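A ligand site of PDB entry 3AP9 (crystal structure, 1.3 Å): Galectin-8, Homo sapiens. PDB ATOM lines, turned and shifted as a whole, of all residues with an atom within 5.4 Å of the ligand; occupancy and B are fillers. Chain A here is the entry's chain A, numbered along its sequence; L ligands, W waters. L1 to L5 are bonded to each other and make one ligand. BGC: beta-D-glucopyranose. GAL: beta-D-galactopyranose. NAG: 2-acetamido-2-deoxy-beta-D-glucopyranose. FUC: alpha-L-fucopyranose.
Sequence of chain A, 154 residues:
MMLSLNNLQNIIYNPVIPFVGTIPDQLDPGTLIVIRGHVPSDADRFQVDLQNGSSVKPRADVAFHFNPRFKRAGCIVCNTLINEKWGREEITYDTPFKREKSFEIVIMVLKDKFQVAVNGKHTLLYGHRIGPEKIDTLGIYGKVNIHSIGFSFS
The side-chain amide oxygen (OE1) of Gln 47 lies within hydrogen-bond range of the guanidinium group (NH2) of Arg 45, 3.1 Å away. N of Gln 47 sits at hydrogen-bond distance from O of Tyr 141. N of Asn 67 sits at hydrogen-bond distance from O of Val 77. The side-chain hydroxyl (OH) of Tyr 141 sits at hydrogen-bond distance from the side-chain amide oxygen (OE1) of Gln 51, at 2.7 Å. The side-chain amide oxygen of Asn 67 is in hydrogen-bond range of the guanidinium group of Arg 45. OE2 of Glu 89 is in salt-bridge range of NH2 of Arg 69 (3.9 Å). ND1 of His 65 sits at hydrogen-bond distance from OD1 of Asp 49 (2.7 Å). The side-chain amide oxygen (OD1) of Asn 67 sits at hydrogen-bond distance from the guanidinium group (NE) of Arg 69 (2.8 Å).
Water W2 lies within hydrogen-bond range of OD2 of Asp 49 (2.7 Å), O2 of GAL L5 (2.8 Å) and OE1 of Gln 51 (2.8 Å). Water W8 lies within hydrogen-bond range of the side-chain carboxylate of Glu 89 (2.7 Å) and an oxygen (O2) of BGC L1 (2.8 Å). Water W15 lies within hydrogen-bond range of O3 of GAL L5 and NE of Arg 59. Water W6 bridges NE2 of Gln 47 (3.0 Å) and O7 of NAG L3 (3.1 Å).
OD1 of Asn 67 lies within hydrogen-bond range of O4 of GAL L2. The side-chain amide nitrogen (NE2) of Gln 47 sits at hydrogen-bond distance from an oxygen (O6) of NAG L3, 2.8 Å away. ND2 of Asn 79 is in hydrogen-bond range of O6 of GAL L2 (2.9 Å). NH1 of Arg 69 lies within hydrogen-bond range of O3 of BGC L1 (2.8 Å). The guanidinium group (NH2) of Arg 59 lies within hydrogen-bond range of an oxygen (O2) of GAL L5 (2.9 Å). NE2 of His 65 lies within hydrogen-bond range of O4 of GAL L2, 2.7 Å away. The side-chain carboxylate (OE2) of Glu 89 lies within hydrogen-bond range of an oxygen (O3) of BGC L1 (2.6 Å). OD2 of Asp 49 sits at hydrogen-bond distance from O6 of NAG L3, 2.6 Å away. The guanidinium group (NH1) of Arg 45 lies within hydrogen-bond range of an oxygen (O4) of GAL L2, 3.0 Å away.
Residues that only touch the ligand: Val 56 (3.995 Å), Trp 86 (3.7 Å) and Tyr 141 (3.4 Å). Hydrophobic or aromatic side chains that line the ligand: Val 56, His 65, Trp 86 and Tyr 141.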
ATOM      1  N   PRO A  18      13.113   8.741   8.766  1.00  0.00           N
ATOM      2  CA  PRO A  18      12.694   9.843   9.639  1.00  0.00           C
ATOM      3  C   PRO A  18      13.744  10.937   9.784  1.00  0.00           C
ATOM      4  O   PRO A  18      14.933  10.657   9.939  1.00  0.00           O
ATOM      5  CB  PRO A  18      12.464   9.152  10.992  1.00  0.00           C
ATOM      6  CG  PRO A  18      13.338   7.964  10.966  1.00  0.00           C
ATOM      7  CD  PRO A  18      13.342   7.500   9.532  1.00  0.00           C
ATOM      8  N   ARG A  45      -0.009   7.392   5.314  1.00  0.00           N
ATOM      9  CA  ARG A  45       0.081   8.633   6.081  1.00  0.00           C
ATOM     10  C   ARG A  45       1.531   9.088   6.213  1.00  0.00           C
ATOM     11  O   ARG A  45       2.453   8.290   6.083  1.00  0.00           O
ATOM     12  CB  ARG A  45      -0.526   8.470   7.490  1.00  0.00           C
ATOM     13  CG  ARG A  45      -0.167   7.160   8.190  1.00  0.00           C
ATOM     14  CD  ARG A  45      -0.591   7.190   9.631  1.00  0.00           C
ATOM     15  NE  ARG A  45       0.265   8.065  10.424  1.00  0.00           N
ATOM     16  CZ  ARG A  45      -0.058   8.585  11.604  1.00  0.00           C
ATOM     17  NH1 ARG A  45      -1.252   8.367  12.147  1.00  0.00           N
ATOM     18  NH2 ARG A  45       0.811   9.346  12.247  1.00  0.00           N
ATOM     19  N   GLN A  47       3.670  12.629   8.517  1.00  0.00           N
ATOM     20  CA  GLN A  47       3.417  13.747   9.416  1.00  0.00           C
ATOM     21  C   GLN A  47       4.628  14.655   9.565  1.00  0.00           C
ATOM     22  O   GLN A  47       5.779  14.232   9.451  1.00  0.00           O
ATOM     23  CB  GLN A  47       2.918  13.285  10.803  1.00  0.00           C
ATOM     24  CG  GLN A  47       3.917  12.458  11.635  1.00  0.00           C
ATOM     25  CD  GLN A  47       3.704  10.960  11.518  1.00  0.00           C
ATOM     26  OE1 GLN A  47       3.174  10.471  10.530  1.00  0.00           O
ATOM     27  NE2 GLN A  47       4.138  10.230  12.532  1.00  0.00           N
ATOM     28  N   ASP A  49       5.931  17.127  12.519  1.00  0.00           N
ATOM     29  CA  ASP A  49       5.799  17.403  13.952  1.00  0.00           C
ATOM     30  C   ASP A  49       6.696  18.556  14.354  1.00  0.00           C
ATOM     31  O   ASP A  49       7.926  18.521  14.134  1.00  0.00           O
ATOM     32  CB  ASP A  49       6.206  16.169  14.784  1.00  0.00           C
ATOM     33  CG  ASP A  49       5.174  15.041  14.747  1.00  0.00           C
ATOM     34  OD1 ASP A  49       4.096  15.196  14.128  1.00  0.00           O
ATOM     35  OD2 ASP A  49       5.442  13.981  15.363  1.00  0.00           O
ATOM     36  N   GLN A  51       8.198  20.170  17.442  1.00  0.00           N
ATOM     37  CA  GLN A  51       8.472  19.575  18.748  1.00  0.00           C
ATOM     38  C   GLN A  51       9.255  20.481  19.672  1.00  0.00           C
ATOM     39  O   GLN A  51      10.053  21.308  19.246  1.00  0.00           O
ATOM     40  CB  GLN A  51       9.287  18.281  18.601  1.00  0.00           C
ATOM     41  CG  GLN A  51       8.692  17.272  17.640  1.00  0.00           C
ATOM     42  CD  GLN A  51       9.482  15.989  17.518  1.00  0.00           C
ATOM     43  OE1 GLN A  51       9.107  15.091  16.778  1.00  0.00           O
ATOM     44  NE2 GLN A  51      10.578  15.888  18.264  1.00  0.00           N
ATOM     45  N   VAL A  56      12.925  10.961  23.380  1.00  0.00           N
ATOM     46  CA  VAL A  56      11.934   9.893  23.315  1.00  0.00           C
ATOM     47  C   VAL A  56      11.571   9.372  24.719  1.00  0.00           C
ATOM     48  O   VAL A  56      10.780   8.444  24.834  1.00  0.00           O
ATOM     49  CB  VAL A  56      12.373   8.731  22.400  1.00  0.00           C
ATOM     50  CG1 VAL A  56      12.558   9.217  20.961  1.00  0.00           C
ATOM     51  CG2 VAL A  56      13.643   8.062  22.925  1.00  0.00           C
ATOM     52  N   ARG A  59       8.685  11.344  25.774  1.00  0.00           N
ATOM     53  CA  ARG A  59       8.573  11.766  24.385  1.00  0.00           C
ATOM     54  C   ARG A  59       8.364  13.270  24.296  1.00  0.00           C
ATOM     55  O   ARG A  59       7.556  13.836  25.032  1.00  0.00           O
ATOM     56  CB  ARG A  59       7.431  11.047  23.698  1.00  0.00           C
ATOM     57  CG  ARG A  59       7.684   9.553  23.605  1.00  0.00           C
ATOM     58  CD  ARG A  59       6.479   8.845  23.080  1.00  0.00           C
ATOM     59  NE  ARG A  59       6.198   9.247  21.702  1.00  0.00           N
ATOM     60  CZ  ARG A  59       5.008   9.168  21.121  1.00  0.00           C
ATOM     61  NH1 ARG A  59       3.937   8.709  21.786  1.00  0.00           N
ATOM     62  NH2 ARG A  59       4.861   9.556  19.869  1.00  0.00           N
ATOM     63  N   VAL A  62       4.726  17.569  21.215  1.00  0.00           N
ATOM     64  CA  VAL A  62       4.490  17.961  19.823  1.00  0.00           C
ATOM     65  C   VAL A  62       3.471  19.089  19.837  1.00  0.00           C
ATOM     66  O   VAL A  62       2.276  18.853  20.024  1.00  0.00           O
ATOM     67  CB  VAL A  62       4.011  16.784  18.958  1.00  0.00           C
ATOM     68  CG1 VAL A  62       3.792  17.248  17.496  1.00  0.00           C
ATOM     69  CG2 VAL A  62       5.005  15.594  19.034  1.00  0.00           C
ATOM     70  N   HIS A  65       1.173  18.597  15.270  1.00  0.00           N
ATOM     71  CA  HIS A  65       1.262  17.342  14.496  1.00  0.00           C
ATOM     72  C   HIS A  65       0.347  17.574  13.303  1.00  0.00           C
ATOM     73  O   HIS A  65      -0.851  17.753  13.480  1.00  0.00           O
ATOM     74  CB  HIS A  65       0.784  16.185  15.389  1.00  0.00           C
ATOM     75  CG  HIS A  65       0.630  14.842  14.729  1.00  0.00           C
ATOM     76  ND1 HIS A  65       1.691  14.028  14.400  1.00  0.00           N
ATOM     77  CD2 HIS A  65      -0.491  14.113  14.468  1.00  0.00           C
ATOM     78  CE1 HIS A  65       1.234  12.870  13.930  1.00  0.00           C
ATOM     79  NE2 HIS A  65      -0.087  12.907  13.950  1.00  0.00           N
ATOM     80  N   ASN A  67      -0.766  15.853   9.921  1.00  0.00           N
ATOM     81  CA  ASN A  67      -0.745  14.430   9.547  1.00  0.00           C
ATOM     82  C   ASN A  67      -1.711  14.086   8.411  1.00  0.00           C
ATOM     83  O   ASN A  67      -2.828  13.656   8.652  1.00  0.00           O
ATOM     84  CB  ASN A  67      -1.047  13.620  10.817  1.00  0.00           C
ATOM     85  CG  ASN A  67      -1.259  12.125  10.603  1.00  0.00           C
ATOM     86  OD1 ASN A  67      -2.081  11.523  11.310  1.00  0.00           O
ATOM     87  ND2 ASN A  67      -0.522  11.516   9.680  1.00  0.00           N
ATOM     88  N   ARG A  69      -3.483  11.869   5.769  1.00  0.00           N
ATOM     89  CA  ARG A  69      -3.849  10.444   5.694  1.00  0.00           C
ATOM     90  C   ARG A  69      -4.519  10.174   4.359  1.00  0.00           C
ATOM     91  O   ARG A  69      -5.264  11.025   3.846  1.00  0.00           O
ATOM     92  CB  ARG A  69      -4.755  10.065   6.850  1.00  0.00           C
ATOM     93  CG  ARG A  69      -4.136  10.310   8.208  1.00  0.00           C
ATOM     94  CD  ARG A  69      -4.996   9.799   9.344  1.00  0.00           C
ATOM     95  NE  ARG A  69      -4.359  10.050  10.631  1.00  0.00           N
ATOM     96  CZ  ARG A  69      -4.870   9.713  11.810  1.00  0.00           C
ATOM     97  NH1 ARG A  69      -6.032   9.072  11.888  1.00  0.00           N
ATOM     98  NH2 ARG A  69      -4.205   9.981  12.928  1.00  0.00           N
ATOM     99  N   VAL A  77      -5.188  15.141   9.619  1.00  0.00           N
ATOM    100  CA  VAL A  77      -5.430  15.187  11.052  1.00  0.00           C
ATOM    101  C   VAL A  77      -4.378  16.063  11.716  1.00  0.00           C
ATOM    102  O   VAL A  77      -3.195  15.915  11.446  1.00  0.00           O
ATOM    103  CB  VAL A  77      -5.403  13.777  11.669  1.00  0.00           C
ATOM    104  CG1 VAL A  77      -5.486  13.843  13.199  1.00  0.00           C
ATOM    105  CG2 VAL A  77      -6.544  12.925  11.094  1.00  0.00           C
ATOM    106  N   CYS A  78      -4.813  16.998  12.564  1.00  0.00           N
ATOM    107  CA  CYS A  78      -3.882  17.797  13.356  1.00  0.00           C
ATOM    108  C   CYS A  78      -4.157  17.580  14.828  1.00  0.00           C
ATOM    109  O   CYS A  78      -5.315  17.408  15.244  1.00  0.00           O
ATOM    110  CB  CYS A  78      -3.983  19.281  12.993  1.00  0.00           C
ATOM    111  SG  CYS A  78      -3.503  19.674  11.295  1.00  0.00           S
ATOM    112  N   ASN A  79      -3.099  17.595  15.641  1.00  0.00           N
ATOM    113  CA  ASN A  79      -3.241  17.418  17.086  1.00  0.00           C
ATOM    114  C   ASN A  79      -1.983  17.895  17.792  1.00  0.00           C
ATOM    115  O   ASN A  79      -1.043  18.388  17.148  1.00  0.00           O
ATOM    116  CB  ASN A  79      -3.511  15.925  17.397  1.00  0.00           C
ATOM    117  CG  ASN A  79      -4.304  15.698  18.699  1.00  0.00           C
ATOM    118  OD1 ASN A  79      -4.442  16.572  19.557  1.00  0.00           O
ATOM    119  ND2 ASN A  79      -4.801  14.476  18.848  1.00  0.00           N
ATOM    120  N   TRP A  86      -2.056  12.523  23.685  1.00  0.00           N
ATOM    121  CA  TRP A  86      -2.703  13.245  22.599  1.00  0.00           C
ATOM    122  C   TRP A  86      -3.924  14.008  23.087  1.00  0.00           C
ATOM    123  O   TRP A  86      -4.667  13.534  23.959  1.00  0.00           O
ATOM    124  CB  TRP A  86      -3.138  12.299  21.489  1.00  0.00           C
ATOM    125  CG  TRP A  86      -2.006  11.773  20.682  1.00  0.00           C
ATOM    126  CD1 TRP A  86      -1.533  10.497  20.662  1.00  0.00           C
ATOM    127  CD2 TRP A  86      -1.176  12.524  19.781  1.00  0.00           C
ATOM    128  NE1 TRP A  86      -0.464  10.398  19.796  1.00  0.00           N
ATOM    129  CE2 TRP A  86      -0.222  11.631  19.246  1.00  0.00           C
ATOM    130  CE3 TRP A  86      -1.158  13.866  19.369  1.00  0.00           C
ATOM    131  CZ2 TRP A  86       0.745  12.036  18.327  1.00  0.00           C
ATOM    132  CZ3 TRP A  86      -0.191  14.262  18.470  1.00  0.00           C
ATOM    133  CH2 TRP A  86       0.745  13.348  17.950  1.00  0.00           C
ATOM    134  N   GLY A  87      -4.136  15.169  22.500  1.00  0.00           N
ATOM    135  CA  GLY A  87      -5.342  15.935  22.730  1.00  0.00           C
ATOM    136  C   GLY A  87      -6.457  15.564  21.777  1.00  0.00           C
ATOM    137  O   GLY A  87      -6.468  14.485  21.190  1.00  0.00           O
ATOM    138  N   GLU A  89      -8.371  15.635  18.373  1.00  0.00           N
ATOM    139  CA  GLU A  89      -8.023  15.773  16.969  1.00  0.00           C
ATOM    140  C   GLU A  89      -8.836  16.863  16.289  1.00  0.00           C
ATOM    141  O   GLU A  89     -10.018  17.066  16.594  1.00  0.00           O
ATOM    142  CB  GLU A  89      -8.278  14.474  16.210  1.00  0.00           C
ATOM    143  CG  GLU A  89      -7.322  13.377  16.588  1.00  0.00           C
ATOM    144  CD  GLU A  89      -7.459  12.110  15.760  1.00  0.00           C
ATOM    145  OE1 GLU A  89      -8.521  11.909  15.108  1.00  0.00           O
ATOM    146  OE2 GLU A  89      -6.502  11.305  15.768  1.00  0.00           O
ATOM    147  N   TYR A 141       8.098  12.357   9.456  1.00  0.00           N
ATOM    148  CA  TYR A 141       7.994  10.927   9.692  1.00  0.00           C
ATOM    149  C   TYR A 141       6.979  10.297   8.736  1.00  0.00           C
ATOM    150  O   TYR A 141       6.075  10.967   8.240  1.00  0.00           O
ATOM    151  CB  TYR A 141       7.515  10.672  11.113  1.00  0.00           C
ATOM    152  CG  TYR A 141       8.291  11.362  12.200  1.00  0.00           C
ATOM    153  CD1 TYR A 141       9.631  11.073  12.410  1.00  0.00           C
ATOM    154  CD2 TYR A 141       7.691  12.282  13.051  1.00  0.00           C
ATOM    155  CE1 TYR A 141      10.339  11.675  13.443  1.00  0.00           C
ATOM    156  CE2 TYR A 141       8.385  12.888  14.081  1.00  0.00           C
ATOM    157  CZ  TYR A 141       9.721  12.592  14.268  1.00  0.00           C
ATOM    158  OH  TYR A 141      10.418  13.185  15.302  1.00  0.00           O
ATOM    159  N   GLY A 142       7.132   8.995   8.519  1.00  0.00           N
ATOM    160  CA  GLY A 142       6.157   8.216   7.750  1.00  0.00           C
ATOM    161  C   GLY A 142       6.507   8.097   6.279  1.00  0.00           C
ATOM    162  O   GLY A 142       7.663   8.239   5.864  1.00  0.00           O
HETATM  163  C2  BGC L   1      -8.086   7.939  16.174  1.00  0.00           C
HETATM  164  C3  BGC L   1      -6.690   7.885  15.567  1.00  0.00           C
HETATM  165  C4  BGC L   1      -5.626   7.905  16.657  1.00  0.00           C
HETATM  166  C5  BGC L   1      -5.912   6.831  17.720  1.00  0.00           C
HETATM  167  C6  BGC L   1      -4.919   6.842  18.879  1.00  0.00           C
HETATM  168  C1  BGC L   1      -8.222   6.854  17.231  1.00  0.00           C
HETATM  169  O1  BGC L   1      -9.530   6.915  17.831  1.00  0.00           O
HETATM  170  O2  BGC L   1      -9.039   7.729  15.131  1.00  0.00           O
HETATM  171  O3  BGC L   1      -6.494   8.978  14.661  1.00  0.00           O
HETATM  172  O4  BGC L   1      -4.365   7.659  16.043  1.00  0.00           O
HETATM  173  O5  BGC L   1      -7.228   7.046  18.236  1.00  0.00           O
HETATM  174  O6  BGC L   1      -4.864   8.124  19.523  1.00  0.00           O
HETATM  175  C1  GAL L   2      -3.314   8.523  16.428  1.00  0.00           C
HETATM  176  C2  GAL L   2      -2.050   8.030  15.757  1.00  0.00           C
HETATM  177  C3  GAL L   2      -0.887   8.989  15.983  1.00  0.00           C
HETATM  178  C4  GAL L   2      -1.305  10.420  15.641  1.00  0.00           C
HETATM  179  C5  GAL L   2      -2.601  10.760  16.376  1.00  0.00           C
HETATM  180  C6  GAL L   2      -3.093  12.161  16.085  1.00  0.00           C
HETATM  181  O2  GAL L   2      -1.697   6.732  16.267  1.00  0.00           O
HETATM  182  O3  GAL L   2       0.215   8.552  15.167  1.00  0.00           O
HETATM  183  O4  GAL L   2      -1.436  10.549  14.229  1.00  0.00           O
HETATM  184  O5  GAL L   2      -3.623   9.841  15.986  1.00  0.00           O
HETATM  185  O6  GAL L   2      -4.289  12.398  16.836  1.00  0.00           O
HETATM  186  C1  NAG L   3       1.467   8.557  15.842  1.00  0.00           C
HETATM  187  C2  NAG L   3       2.338   7.418  15.334  1.00  0.00           C
HETATM  188  C3  NAG L   3       3.659   7.459  16.088  1.00  0.00           C
HETATM  189  C4  NAG L   3       4.294   8.859  15.980  1.00  0.00           C
HETATM  190  C5  NAG L   3       3.275   9.935  16.387  1.00  0.00           C
HETATM  191  C6  NAG L   3       3.809  11.357  16.288  1.00  0.00           C
HETATM  192  C7  NAG L   3       1.149   5.452  14.518  1.00  0.00           C
HETATM  193  C8  NAG L   3       0.417   4.165  14.776  1.00  0.00           C
HETATM  194  N2  NAG L   3       1.643   6.150  15.556  1.00  0.00           N
HETATM  195  O3  NAG L   3       4.597   6.512  15.583  1.00  0.00           O
HETATM  196  O4  NAG L   3       5.387   8.949  16.875  1.00  0.00           O
HETATM  197  O5  NAG L   3       2.097   9.812  15.590  1.00  0.00           O
HETATM  198  O6  NAG L   3       4.351  11.636  14.990  1.00  0.00           O
HETATM  199  O7  NAG L   3       1.310   5.839  13.378  1.00  0.00           O
HETATM  200  C1  FUC L   4       4.617   5.235  16.255  1.00  0.00           C
HETATM  201  C2  FUC L   4       5.707   4.363  15.650  1.00  0.00           C
HETATM  202  C3  FUC L   4       7.089   4.907  16.008  1.00  0.00           C
HETATM  203  C4  FUC L   4       7.228   5.059  17.512  1.00  0.00           C
HETATM  204  C5  FUC L   4       6.104   5.911  18.069  1.00  0.00           C
HETATM  205  C6  FUC L   4       6.161   5.987  19.593  1.00  0.00           C
HETATM  206  O2  FUC L   4       5.535   4.311  14.230  1.00  0.00           O
HETATM  207  O3  FUC L   4       8.111   4.049  15.522  1.00  0.00           O
HETATM  208  O4  FUC L   4       7.207   3.760  18.130  1.00  0.00           O
HETATM  209  O5  FUC L   4       4.838   5.371  17.673  1.00  0.00           O
HETATM  210  C1  GAL L   5       6.615   9.408  16.318  1.00  0.00           C
HETATM  211  C2  GAL L   5       7.583   9.632  17.479  1.00  0.00           C
HETATM  212  C3  GAL L   5       8.979   9.978  16.994  1.00  0.00           C
HETATM  213  C4  GAL L   5       9.424   8.940  15.963  1.00  0.00           C
HETATM  214  C5  GAL L   5       8.380   8.788  14.868  1.00  0.00           C
HETATM  215  C6  GAL L   5       8.820   7.736  13.866  1.00  0.00           C
HETATM  216  O2  GAL L   5       7.078  10.650  18.349  1.00  0.00           O
HETATM  217  O3  GAL L   5       9.899  10.025  18.091  1.00  0.00           O
HETATM  218  O4  GAL L   5       9.614   7.680  16.608  1.00  0.00           O
HETATM  219  O5  GAL L   5       7.111   8.420  15.427  1.00  0.00           O
HETATM  220  O6  GAL L   5       7.886   7.707  12.791  1.00  0.00           O
HETATM  221  O   HOH W   1       1.494   5.429  18.409  1.00  0.00           O
HETATM  222  O   HOH W   2       7.055  13.255  17.440  1.00  0.00           O
HETATM  223  O   HOH W   3      -3.198   4.653  15.098  1.00  0.00           O
HETATM  224  O   HOH W   4      -3.802   7.975  22.021  1.00  0.00           O
HETATM  225  O   HOH W   5       4.875   2.390  18.800  1.00  0.00           O
HETATM  226  O   HOH W   6       3.770   7.263  12.152  1.00  0.00           O
HETATM  227  O   HOH W   7       5.818   6.016  12.524  1.00  0.00           O
HETATM  228  O   HOH W   8      -9.358   9.908  13.463  1.00  0.00           O
HETATM  229  O   HOH W   9       8.483   1.496  16.439  1.00  0.00           O
HETATM  230  O   HOH W  10      12.212   7.063  17.843  1.00  0.00           O
HETATM  231  O   HOH W  11      -1.028   6.776  18.863  1.00  0.00           O
HETATM  232  O   HOH W  12      10.138  12.215  19.926  1.00  0.00           O
HETATM  233  O   HOH W  13      -5.379  10.825  19.143  1.00  0.00           O
HETATM  234  O   HOH W  14       7.419  13.225  20.372  1.00  0.00           O
HETATM  235  O   HOH W  15       9.007   8.524  20.390  1.00  0.00           O
HETATM  236  O   HOH W  16     -11.860   7.247  16.256  1.00  0.00           O
